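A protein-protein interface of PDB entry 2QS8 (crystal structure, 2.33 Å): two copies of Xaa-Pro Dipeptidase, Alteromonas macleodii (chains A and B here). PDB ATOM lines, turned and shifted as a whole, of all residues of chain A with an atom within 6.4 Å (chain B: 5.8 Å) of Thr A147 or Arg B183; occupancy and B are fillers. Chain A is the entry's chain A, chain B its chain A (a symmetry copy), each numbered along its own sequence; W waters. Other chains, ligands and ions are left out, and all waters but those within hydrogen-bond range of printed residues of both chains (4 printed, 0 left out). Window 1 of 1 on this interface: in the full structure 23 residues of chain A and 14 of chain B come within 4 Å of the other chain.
Thr A147 touches two residues of chain B.
Arg B183 touches just these residues of chain A: Thr A146 (3.5 Å), Thr A147 (3.3 Å), Asn A173 (2.9 Å), Gln A212 (3.2 Å), Thr A214 (3.8 Å) and Glu A217 (2.9 Å).
Of the printed residues of chain B, Gly A148 touches Tyr B186 (3.4 Å) and Lys B187 (3.8 Å).
Of the printed residues of chain B, Glu A217 touches Arg B183.
Of the printed residues of chain B, Asn A155 touches Lys B187 (3.5 Å).
The nearest printed residue of chain A that does not touch Asp B227 is Thr A214 (4.6 Å).
No position is printed for both chains.
Of the 17 pairs that touch across the chains among the printed residues, none has its exchanged pair printed and touching as well.
Hydrophobic or aromatic side chains of chain B that line the printed part of chain A: Tyr B179, Ala B180, Tyr B186 and Tyr B228.
Along chain B the printed residues that touch a printed residue of chain A span positions 179 to 228.
Among the printed residues, 17 pairs touch across the chains.
CG2 of Thr A146 touches NH1 of Arg B183 (3.5 Å).
OG1 of Thr A146 touches OH of Tyr B228 (3.6 Å).
Thr A147 touches Gln B184 (CG2 to OE1, 3.5 Å).
Tyr B186 touches Gly A148.
Gly A148 touches Lys B187.
Asn A155 touches Lys B187 (OD1 to CG, 3.5 Å).
CD of Pro A211 touches O of Asp B227, 3.4 Å away.
CA of Gln A212 touches OH of Tyr B228, 3.5 Å away.
Tyr B179 touches Thr A214 (CE2 to CG2, 3.4 Å).
NH2 of Arg B183 touches CG2 of Thr A214 (3.8 Å).
Water W3 lies within hydrogen-bond range of the backbone carbonyl oxygen of Gly A148, the side-chain hydroxyl of Tyr B186 and the side-chain amide nitrogen of Gln A212.
Water W1 bridges OG1 of Thr A147 (2.6 Å) and OE2 of Glu B168 (2.6 Å).
Water W2 lies within hydrogen-bond range of OG1 of Thr A146 (2.6 Å), OH of Tyr B228 (2.7 Å), O of Thr A147 (2.9 Å) and N of Gly A149 (3.1 Å).
Water W4 lies within hydrogen-bond range of the side-chain carboxylate of Asp B227 (2.9 Å), the guanidinium group of Arg B183 (2.9 Å), the backbone carbonyl oxygen of Pro A211 (3.0 Å) and the backbone NH of Phe A213 (3.4 Å).
OG1 of Thr A146 lies within hydrogen-bond range of O of Gln A212 (2.7 Å).
The backbone NH of Gly A148 sits at hydrogen-bond distance from the side-chain carboxylate of Asp A152 (2.9 Å).
The side-chain amide nitrogen (ND2) of Asn A155 sits at hydrogen-bond distance from the backbone carbonyl oxygen (O) of Gly A149 (2.9 Å).
The backbone NH (N) of Gly A174 is in hydrogen-bond range of the side-chain carboxylate (OE2) of Glu A217 (2.6 Å).
The side-chain hydroxyl (OG1) of Thr A214 is in hydrogen-bond range of the backbone NH (N) of Glu A217 (2.9 Å).
The side-chain hydroxyl (OH) of Tyr B228 sits at hydrogen-bond distance from the guanidinium group (NE) of Arg B183, at 2.8 Å.
The side-chain carboxylate (OD2) of Asp A152 lies within salt-bridge range of the side-chain amino group (NZ) of Lys B187, at 2.7 Å.
OD1 of Asn A173 is in hydrogen-bond range of NH1 of Arg B183, 2.9 Å away.
NH2 of Arg B183 sits at hydrogen-bond distance from O of Gln A212 (3.2 Å).
NH2 of Arg B183 lies within salt-bridge range of OE1 of Glu A217, at 2.9 Å.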
ATOM      1  N   ALA A 145      21.172 -10.443 -33.775  1.00  0.00           N
ATOM      2  CA  ALA A 145      20.199 -11.447 -33.387  1.00  0.00           C
ATOM      3  C   ALA A 145      18.883 -10.820 -32.944  1.00  0.00           C
ATOM      4  O   ALA A 145      18.787  -9.604 -32.738  1.00  0.00           O
ATOM      5  CB  ALA A 145      20.763 -12.294 -32.237  1.00  0.00           C
ATOM      6  N   THR A 146      17.869 -11.670 -32.805  1.00  0.00           N
ATOM      7  CA  THR A 146      16.570 -11.238 -32.318  1.00  0.00           C
ATOM      8  C   THR A 146      16.522 -11.592 -30.827  1.00  0.00           C
ATOM      9  O   THR A 146      17.317 -12.399 -30.355  1.00  0.00           O
ATOM     10  CB  THR A 146      15.421 -11.944 -33.052  1.00  0.00           C
ATOM     11  OG1 THR A 146      15.624 -13.358 -33.044  1.00  0.00           O
ATOM     12  CG2 THR A 146      15.358 -11.450 -34.475  1.00  0.00           C
ATOM     13  N   THR A 147      15.593 -10.984 -30.098  1.00  0.00           N
ATOM     14  CA  THR A 147      15.475 -11.234 -28.663  1.00  0.00           C
ATOM     15  C   THR A 147      15.610 -12.711 -28.291  1.00  0.00           C
ATOM     16  O   THR A 147      14.867 -13.555 -28.777  1.00  0.00           O
ATOM     17  CB  THR A 147      14.139 -10.702 -28.127  1.00  0.00           C
ATOM     18  OG1 THR A 147      14.103  -9.278 -28.295  1.00  0.00           O
ATOM     19  CG2 THR A 147      13.958 -11.071 -26.634  1.00  0.00           C
ATOM     20  N   GLY A 148      16.569 -13.012 -27.424  1.00  0.00           N
ATOM     21  CA  GLY A 148      16.769 -14.386 -26.999  1.00  0.00           C
ATOM     22  C   GLY A 148      17.519 -15.261 -27.986  1.00  0.00           C
ATOM     23  O   GLY A 148      17.806 -16.419 -27.696  1.00  0.00           O
ATOM     24  N   GLY A 149      17.841 -14.700 -29.146  1.00  0.00           N
ATOM     25  CA  GLY A 149      18.545 -15.437 -30.177  1.00  0.00           C
ATOM     26  C   GLY A 149      19.939 -15.903 -29.801  1.00  0.00           C
ATOM     27  O   GLY A 149      20.542 -15.436 -28.823  1.00  0.00           O
ATOM     28  N   ASP A 152      22.280 -13.225 -28.769  1.00  0.00           N
ATOM     29  CA  ASP A 152      21.821 -12.187 -27.853  1.00  0.00           C
ATOM     30  C   ASP A 152      22.820 -12.243 -26.694  1.00  0.00           C
ATOM     31  O   ASP A 152      22.885 -13.231 -25.957  1.00  0.00           O
ATOM     32  CB  ASP A 152      20.411 -12.500 -27.344  1.00  0.00           C
ATOM     33  CG  ASP A 152      19.873 -11.428 -26.392  1.00  0.00           C
ATOM     34  OD1 ASP A 152      20.688 -10.749 -25.733  1.00  0.00           O
ATOM     35  OD2 ASP A 152      18.634 -11.281 -26.294  1.00  0.00           O
ATOM     36  N   ASN A 155      21.578 -13.299 -22.893  1.00  0.00           N
ATOM     37  CA  ASN A 155      21.005 -14.599 -22.540  1.00  0.00           C
ATOM     38  C   ASN A 155      21.752 -15.122 -21.315  1.00  0.00           C
ATOM     39  O   ASN A 155      22.848 -14.665 -21.011  1.00  0.00           O
ATOM     40  CB  ASN A 155      21.170 -15.612 -23.677  1.00  0.00           C
ATOM     41  CG  ASN A 155      20.088 -15.490 -24.744  1.00  0.00           C
ATOM     42  OD1 ASN A 155      18.951 -15.127 -24.462  1.00  0.00           O
ATOM     43  ND2 ASN A 155      20.441 -15.825 -25.976  1.00  0.00           N
ATOM     44  N   PRO A 165      18.377  -5.266 -24.398  1.00  0.00           N
ATOM     45  CA  PRO A 165      19.216  -4.687 -25.451  1.00  0.00           C
ATOM     46  C   PRO A 165      18.436  -3.878 -26.473  1.00  0.00           C
ATOM     47  O   PRO A 165      17.257  -4.137 -26.718  1.00  0.00           O
ATOM     48  CB  PRO A 165      19.864  -5.908 -26.097  1.00  0.00           C
ATOM     49  CG  PRO A 165      19.730  -6.990 -25.053  1.00  0.00           C
ATOM     50  CD  PRO A 165      18.384  -6.735 -24.481  1.00  0.00           C
ATOM     51  N   VAL A 171      20.555  -6.636 -31.039  1.00  0.00           N
ATOM     52  CA  VAL A 171      19.351  -7.425 -30.758  1.00  0.00           C
ATOM     53  C   VAL A 171      18.162  -6.659 -31.345  1.00  0.00           C
ATOM     54  O   VAL A 171      17.859  -5.532 -30.942  1.00  0.00           O
ATOM     55  CB  VAL A 171      19.152  -7.654 -29.251  1.00  0.00           C
ATOM     56  CG1 VAL A 171      18.005  -8.663 -29.019  1.00  0.00           C
ATOM     57  CG2 VAL A 171      20.456  -8.169 -28.644  1.00  0.00           C
ATOM     58  N   VAL A 172      17.496  -7.287 -32.308  1.00  0.00           N
ATOM     59  CA  VAL A 172      16.409  -6.652 -33.043  1.00  0.00           C
ATOM     60  C   VAL A 172      15.102  -7.426 -33.154  1.00  0.00           C
ATOM     61  O   VAL A 172      15.043  -8.627 -32.910  1.00  0.00           O
ATOM     62  CB  VAL A 172      16.863  -6.383 -34.490  1.00  0.00           C
ATOM     63  CG1 VAL A 172      18.122  -5.529 -34.500  1.00  0.00           C
ATOM     64  CG2 VAL A 172      17.125  -7.719 -35.188  1.00  0.00           C
ATOM     65  N   ASN A 173      14.066  -6.703 -33.565  1.00  0.00           N
ATOM     66  CA  ASN A 173      12.734  -7.249 -33.792  1.00  0.00           C
ATOM     67  C   ASN A 173      12.109  -6.363 -34.877  1.00  0.00           C
ATOM     68  O   ASN A 173      11.989  -5.150 -34.699  1.00  0.00           O
ATOM     69  CB  ASN A 173      11.888  -7.204 -32.511  1.00  0.00           C
ATOM     70  CG  ASN A 173      12.356  -8.196 -31.466  1.00  0.00           C
ATOM     71  OD1 ASN A 173      12.281  -9.416 -31.663  1.00  0.00           O
ATOM     72  ND2 ASN A 173      12.849  -7.682 -30.343  1.00  0.00           N
ATOM     73  N   GLY A 174      11.737  -6.968 -36.001  1.00  0.00           N
ATOM     74  CA  GLY A 174      11.145  -6.214 -37.092  1.00  0.00           C
ATOM     75  C   GLY A 174      12.187  -5.691 -38.064  1.00  0.00           C
ATOM     76  O   GLY A 174      13.371  -5.625 -37.729  1.00  0.00           O
ATOM     77  N   PRO A 211      13.987 -21.343 -36.300  1.00  0.00           N
ATOM     78  CA  PRO A 211      14.100 -20.119 -37.116  1.00  0.00           C
ATOM     79  C   PRO A 211      13.924 -18.871 -36.230  1.00  0.00           C
ATOM     80  O   PRO A 211      12.873 -18.697 -35.596  1.00  0.00           O
ATOM     81  CB  PRO A 211      12.970 -20.283 -38.129  1.00  0.00           C
ATOM     82  CG  PRO A 211      11.926 -21.013 -37.331  1.00  0.00           C
ATOM     83  CD  PRO A 211      12.740 -22.064 -36.608  1.00  0.00           C
ATOM     84  N   GLN A 212      14.946 -18.017 -36.179  1.00  0.00           N
ATOM     85  CA  GLN A 212      14.890 -16.820 -35.329  1.00  0.00           C
ATOM     86  C   GLN A 212      14.813 -15.470 -36.057  1.00  0.00           C
ATOM     87  O   GLN A 212      14.877 -14.411 -35.439  1.00  0.00           O
ATOM     88  CB  GLN A 212      16.054 -16.837 -34.334  1.00  0.00           C
ATOM     89  CG  GLN A 212      16.106 -18.133 -33.533  1.00  0.00           C
ATOM     90  CD  GLN A 212      17.120 -18.102 -32.412  1.00  0.00           C
ATOM     91  OE1 GLN A 212      18.136 -17.407 -32.500  1.00  0.00           O
ATOM     92  NE2 GLN A 212      16.861 -18.875 -31.357  1.00  0.00           N
ATOM     93  N   PHE A 213      14.668 -15.519 -37.371  1.00  0.00           N
ATOM     94  CA  PHE A 213      14.506 -14.321 -38.184  1.00  0.00           C
ATOM     95  C   PHE A 213      13.296 -14.596 -39.069  1.00  0.00           C
ATOM     96  O   PHE A 213      13.158 -15.697 -39.613  1.00  0.00           O
ATOM     97  CB  PHE A 213      15.730 -14.065 -39.071  1.00  0.00           C
ATOM     98  CG  PHE A 213      16.749 -13.119 -38.476  1.00  0.00           C
ATOM     99  CD1 PHE A 213      17.559 -13.509 -37.414  1.00  0.00           C
ATOM    100  CD2 PHE A 213      16.895 -11.836 -38.989  1.00  0.00           C
ATOM    101  CE1 PHE A 213      18.507 -12.633 -36.873  1.00  0.00           C
ATOM    102  CE2 PHE A 213      17.839 -10.946 -38.455  1.00  0.00           C
ATOM    103  CZ  PHE A 213      18.646 -11.348 -37.395  1.00  0.00           C
ATOM    104  N   THR A 214      12.409 -13.621 -39.200  1.00  0.00           N
ATOM    105  CA  THR A 214      11.242 -13.782 -40.063  1.00  0.00           C
ATOM    106  C   THR A 214      11.774 -13.497 -41.473  1.00  0.00           C
ATOM    107  O   THR A 214      12.869 -12.955 -41.625  1.00  0.00           O
ATOM    108  CB  THR A 214      10.150 -12.753 -39.735  1.00  0.00           C
ATOM    109  OG1 THR A 214      10.632 -11.458 -40.092  1.00  0.00           O
ATOM    110  CG2 THR A 214       9.802 -12.759 -38.225  1.00  0.00           C
ATOM    111  N   GLU A 217      12.363  -9.891 -41.797  1.00  0.00           N
ATOM    112  CA  GLU A 217      13.538  -9.438 -41.075  1.00  0.00           C
ATOM    113  C   GLU A 217      14.852  -9.785 -41.792  1.00  0.00           C
ATOM    114  O   GLU A 217      15.744  -8.945 -41.877  1.00  0.00           O
ATOM    115  CB  GLU A 217      13.550 -10.003 -39.644  1.00  0.00           C
ATOM    116  CG  GLU A 217      12.377  -9.543 -38.773  1.00  0.00           C
ATOM    117  CD  GLU A 217      12.331 -10.224 -37.406  1.00  0.00           C
ATOM    118  OE1 GLU A 217      12.666 -11.419 -37.296  1.00  0.00           O
ATOM    119  OE2 GLU A 217      11.930  -9.560 -36.433  1.00  0.00           O
ATOM    120  N   GLU B 168       9.105  -6.345 -23.813  1.00  0.00           N
ATOM    121  CA  GLU B 168       9.712  -7.464 -23.111  1.00  0.00           C
ATOM    122  C   GLU B 168       9.013  -7.757 -21.784  1.00  0.00           C
ATOM    123  O   GLU B 168       9.104  -8.859 -21.275  1.00  0.00           O
ATOM    124  CB  GLU B 168      11.210  -7.209 -22.882  1.00  0.00           C
ATOM    125  CG  GLU B 168      12.070  -7.233 -24.148  1.00  0.00           C
ATOM    126  CD  GLU B 168      12.186  -5.883 -24.842  1.00  0.00           C
ATOM    127  OE1 GLU B 168      11.338  -4.987 -24.604  1.00  0.00           O
ATOM    128  OE2 GLU B 168      13.131  -5.717 -25.644  1.00  0.00           O
ATOM    129  N   VAL B 178       5.006  -7.352 -30.650  1.00  0.00           N
ATOM    130  CA  VAL B 178       4.480  -8.675 -30.330  1.00  0.00           C
ATOM    131  C   VAL B 178       5.611  -9.704 -30.387  1.00  0.00           C
ATOM    132  O   VAL B 178       5.753 -10.512 -29.470  1.00  0.00           O
ATOM    133  CB  VAL B 178       3.357  -9.115 -31.299  1.00  0.00           C
ATOM    134  CG1 VAL B 178       3.184 -10.651 -31.272  1.00  0.00           C
ATOM    135  CG2 VAL B 178       2.055  -8.480 -30.888  1.00  0.00           C
ATOM    136  N   TYR B 179       6.414  -9.665 -31.456  1.00  0.00           N
ATOM    137  CA  TYR B 179       7.522 -10.604 -31.606  1.00  0.00           C
ATOM    138  C   TYR B 179       8.538 -10.453 -30.468  1.00  0.00           C
ATOM    139  O   TYR B 179       9.057 -11.444 -29.957  1.00  0.00           O
ATOM    140  CB  TYR B 179       8.228 -10.414 -32.960  1.00  0.00           C
ATOM    141  CG  TYR B 179       7.721 -11.325 -34.062  1.00  0.00           C
ATOM    142  CD1 TYR B 179       6.558 -11.017 -34.772  1.00  0.00           C
ATOM    143  CD2 TYR B 179       8.411 -12.497 -34.399  1.00  0.00           C
ATOM    144  CE1 TYR B 179       6.098 -11.849 -35.792  1.00  0.00           C
ATOM    145  CE2 TYR B 179       7.959 -13.340 -35.420  1.00  0.00           C
ATOM    146  CZ  TYR B 179       6.805 -13.010 -36.108  1.00  0.00           C
ATOM    147  OH  TYR B 179       6.367 -13.844 -37.105  1.00  0.00           O
ATOM    148  N   ALA B 180       8.822  -9.215 -30.081  1.00  0.00           N
ATOM    149  CA  ALA B 180       9.757  -8.969 -29.002  1.00  0.00           C
ATOM    150  C   ALA B 180       9.230  -9.651 -27.752  1.00  0.00           C
ATOM    151  O   ALA B 180       9.980 -10.321 -27.046  1.00  0.00           O
ATOM    152  CB  ALA B 180       9.913  -7.469 -28.755  1.00  0.00           C
ATOM    153  N   ALA B 181       7.936  -9.493 -27.493  1.00  0.00           N
ATOM    154  CA  ALA B 181       7.299 -10.087 -26.318  1.00  0.00           C
ATOM    155  C   ALA B 181       7.267 -11.625 -26.349  1.00  0.00           C
ATOM    156  O   ALA B 181       7.473 -12.274 -25.320  1.00  0.00           O
ATOM    157  CB  ALA B 181       5.879  -9.536 -26.155  1.00  0.00           C
ATOM    158  N   VAL B 182       6.988 -12.205 -27.510  1.00  0.00           N
ATOM    159  CA  VAL B 182       6.954 -13.653 -27.626  1.00  0.00           C
ATOM    160  C   VAL B 182       8.373 -14.195 -27.439  1.00  0.00           C
ATOM    161  O   VAL B 182       8.589 -15.137 -26.696  1.00  0.00           O
ATOM    162  CB  VAL B 182       6.404 -14.098 -29.000  1.00  0.00           C
ATOM    163  CG1 VAL B 182       6.617 -15.590 -29.205  1.00  0.00           C
ATOM    164  CG2 VAL B 182       4.927 -13.771 -29.083  1.00  0.00           C
ATOM    165  N   ARG B 183       9.337 -13.583 -28.114  1.00  0.00           N
ATOM    166  CA  ARG B 183      10.717 -14.004 -27.987  1.00  0.00           C
ATOM    167  C   ARG B 183      11.235 -13.857 -26.551  1.00  0.00           C
ATOM    168  O   ARG B 183      12.048 -14.670 -26.102  1.00  0.00           O
ATOM    169  CB  ARG B 183      11.592 -13.230 -28.975  1.00  0.00           C
ATOM    170  CG  ARG B 183      11.429 -13.730 -30.422  1.00  0.00           C
ATOM    171  CD  ARG B 183      12.094 -12.816 -31.444  1.00  0.00           C
ATOM    172  NE  ARG B 183      12.026 -13.356 -32.800  1.00  0.00           N
ATOM    173  CZ  ARG B 183      11.970 -12.607 -33.898  1.00  0.00           C
ATOM    174  NH1 ARG B 183      11.973 -11.280 -33.808  1.00  0.00           N
ATOM    175  NH2 ARG B 183      11.907 -13.172 -35.086  1.00  0.00           N
ATOM    176  N   GLN B 184      10.752 -12.841 -25.824  1.00  0.00           N
ATOM    177  CA  GLN B 184      11.175 -12.648 -24.439  1.00  0.00           C
ATOM    178  C   GLN B 184      10.714 -13.824 -23.579  1.00  0.00           C
ATOM    179  O   GLN B 184      11.418 -14.251 -22.665  1.00  0.00           O
ATOM    180  CB  GLN B 184      10.593 -11.353 -23.855  1.00  0.00           C
ATOM    181  CG  GLN B 184      11.081 -11.043 -22.454  1.00  0.00           C
ATOM    182  CD  GLN B 184      12.588 -10.865 -22.403  1.00  0.00           C
ATOM    183  OE1 GLN B 184      13.182 -10.266 -23.301  1.00  0.00           O
ATOM    184  NE2 GLN B 184      13.214 -11.375 -21.344  1.00  0.00           N
ATOM    185  N   ARG B 185       9.523 -14.340 -23.870  1.00  0.00           N
ATOM    186  CA  ARG B 185       9.018 -15.475 -23.109  1.00  0.00           C
ATOM    187  C   ARG B 185       9.890 -16.698 -23.414  1.00  0.00           C
ATOM    188  O   ARG B 185      10.157 -17.510 -22.535  1.00  0.00           O
ATOM    189  CB  ARG B 185       7.545 -15.728 -23.442  1.00  0.00           C
ATOM    190  CG  ARG B 185       6.591 -15.361 -22.300  1.00  0.00           C
ATOM    191  CD  ARG B 185       7.155 -14.257 -21.397  1.00  0.00           C
ATOM    192  NE  ARG B 185       6.967 -12.939 -21.969  1.00  0.00           N
ATOM    193  CZ  ARG B 185       7.551 -11.830 -21.539  1.00  0.00           C
ATOM    194  NH1 ARG B 185       8.387 -11.846 -20.514  1.00  0.00           N
ATOM    195  NH2 ARG B 185       7.288 -10.688 -22.154  1.00  0.00           N
ATOM    196  N   TYR B 186      10.330 -16.815 -24.662  1.00  0.00           N
ATOM    197  CA  TYR B 186      11.217 -17.908 -25.044  1.00  0.00           C
ATOM    198  C   TYR B 186      12.528 -17.734 -24.257  1.00  0.00           C
ATOM    199  O   TYR B 186      13.109 -18.695 -23.750  1.00  0.00           O
ATOM    200  CB  TYR B 186      11.529 -17.839 -26.549  1.00  0.00           C
ATOM    201  CG  TYR B 186      12.791 -18.553 -26.957  1.00  0.00           C
ATOM    202  CD1 TYR B 186      12.866 -19.951 -26.963  1.00  0.00           C
ATOM    203  CD2 TYR B 186      13.924 -17.835 -27.331  1.00  0.00           C
ATOM    204  CE1 TYR B 186      14.042 -20.611 -27.333  1.00  0.00           C
ATOM    205  CE2 TYR B 186      15.100 -18.479 -27.702  1.00  0.00           C
ATOM    206  CZ  TYR B 186      15.154 -19.866 -27.704  1.00  0.00           C
ATOM    207  OH  TYR B 186      16.312 -20.496 -28.087  1.00  0.00           O
ATOM    208  N   LYS B 187      12.965 -16.485 -24.162  1.00  0.00           N
ATOM    209  CA  LYS B 187      14.199 -16.150 -23.471  1.00  0.00           C
ATOM    210  C   LYS B 187      14.092 -16.461 -21.984  1.00  0.00           C
ATOM    211  O   LYS B 187      15.035 -16.977 -21.409  1.00  0.00           O
ATOM    212  CB  LYS B 187      14.533 -14.665 -23.697  1.00  0.00           C
ATOM    213  CG  LYS B 187      15.886 -14.187 -23.168  1.00  0.00           C
ATOM    214  CD  LYS B 187      16.153 -12.739 -23.622  1.00  0.00           C
ATOM    215  CE  LYS B 187      17.449 -12.201 -23.033  1.00  0.00           C
ATOM    216  NZ  LYS B 187      17.853 -10.942 -23.691  1.00  0.00           N
ATOM    217  N   ASP B 188      12.944 -16.168 -21.373  1.00  0.00           N
ATOM    218  CA  ASP B 188      12.758 -16.435 -19.952  1.00  0.00           C
ATOM    219  C   ASP B 188      12.708 -17.938 -19.648  1.00  0.00           C
ATOM    220  O   ASP B 188      12.933 -18.344 -18.511  1.00  0.00           O
ATOM    221  CB  ASP B 188      11.474 -15.790 -19.428  1.00  0.00           C
ATOM    222  CG  ASP B 188      11.496 -14.270 -19.506  1.00  0.00           C
ATOM    223  OD1 ASP B 188      12.583 -13.663 -19.376  1.00  0.00           O
ATOM    224  OD2 ASP B 188      10.412 -13.686 -19.677  1.00  0.00           O
ATOM    225  N   ASP B 227       7.405 -20.178 -34.899  1.00  0.00           N
ATOM    226  CA  ASP B 227       8.848 -20.222 -35.141  1.00  0.00           C
ATOM    227  C   ASP B 227       9.607 -20.741 -33.923  1.00  0.00           C
ATOM    228  O   ASP B 227      10.718 -21.240 -34.050  1.00  0.00           O
ATOM    229  CB  ASP B 227       9.394 -18.835 -35.506  1.00  0.00           C
ATOM    230  CG  ASP B 227       9.085 -18.434 -36.947  1.00  0.00           C
ATOM    231  OD1 ASP B 227       8.555 -19.267 -37.723  1.00  0.00           O
ATOM    232  OD2 ASP B 227       9.388 -17.273 -37.298  1.00  0.00           O
ATOM    233  N   TYR B 228       9.013 -20.628 -32.743  1.00  0.00           N
ATOM    234  CA  TYR B 228       9.692 -21.099 -31.552  1.00  0.00           C
ATOM    235  C   TYR B 228       9.089 -22.387 -30.990  1.00  0.00           C
ATOM    236  O   TYR B 228       9.430 -22.811 -29.888  1.00  0.00           O
ATOM    237  CB  TYR B 228       9.726 -19.979 -30.493  1.00  0.00           C
ATOM    238  CG  TYR B 228      10.617 -18.826 -30.918  1.00  0.00           C
ATOM    239  CD1 TYR B 228      10.208 -17.938 -31.920  1.00  0.00           C
ATOM    240  CD2 TYR B 228      11.913 -18.698 -30.412  1.00  0.00           C
ATOM    241  CE1 TYR B 228      11.067 -16.965 -32.415  1.00  0.00           C
ATOM    242  CE2 TYR B 228      12.787 -17.722 -30.906  1.00  0.00           C
ATOM    243  CZ  TYR B 228      12.352 -16.863 -31.912  1.00  0.00           C
ATOM    244  OH  TYR B 228      13.197 -15.919 -32.431  1.00  0.00           O
HETATM  245  O   HOH W   1      14.741  -7.568 -26.475  1.00  0.00           O
HETATM  246  O   HOH W   2      15.448 -15.107 -31.115  1.00  0.00           O
HETATM  247  O   HOH W   3      18.105 -18.694 -28.781  1.00  0.00           O
HETATM  248  O   HOH W   4      11.592 -15.976 -35.934  1.00  0.00           O
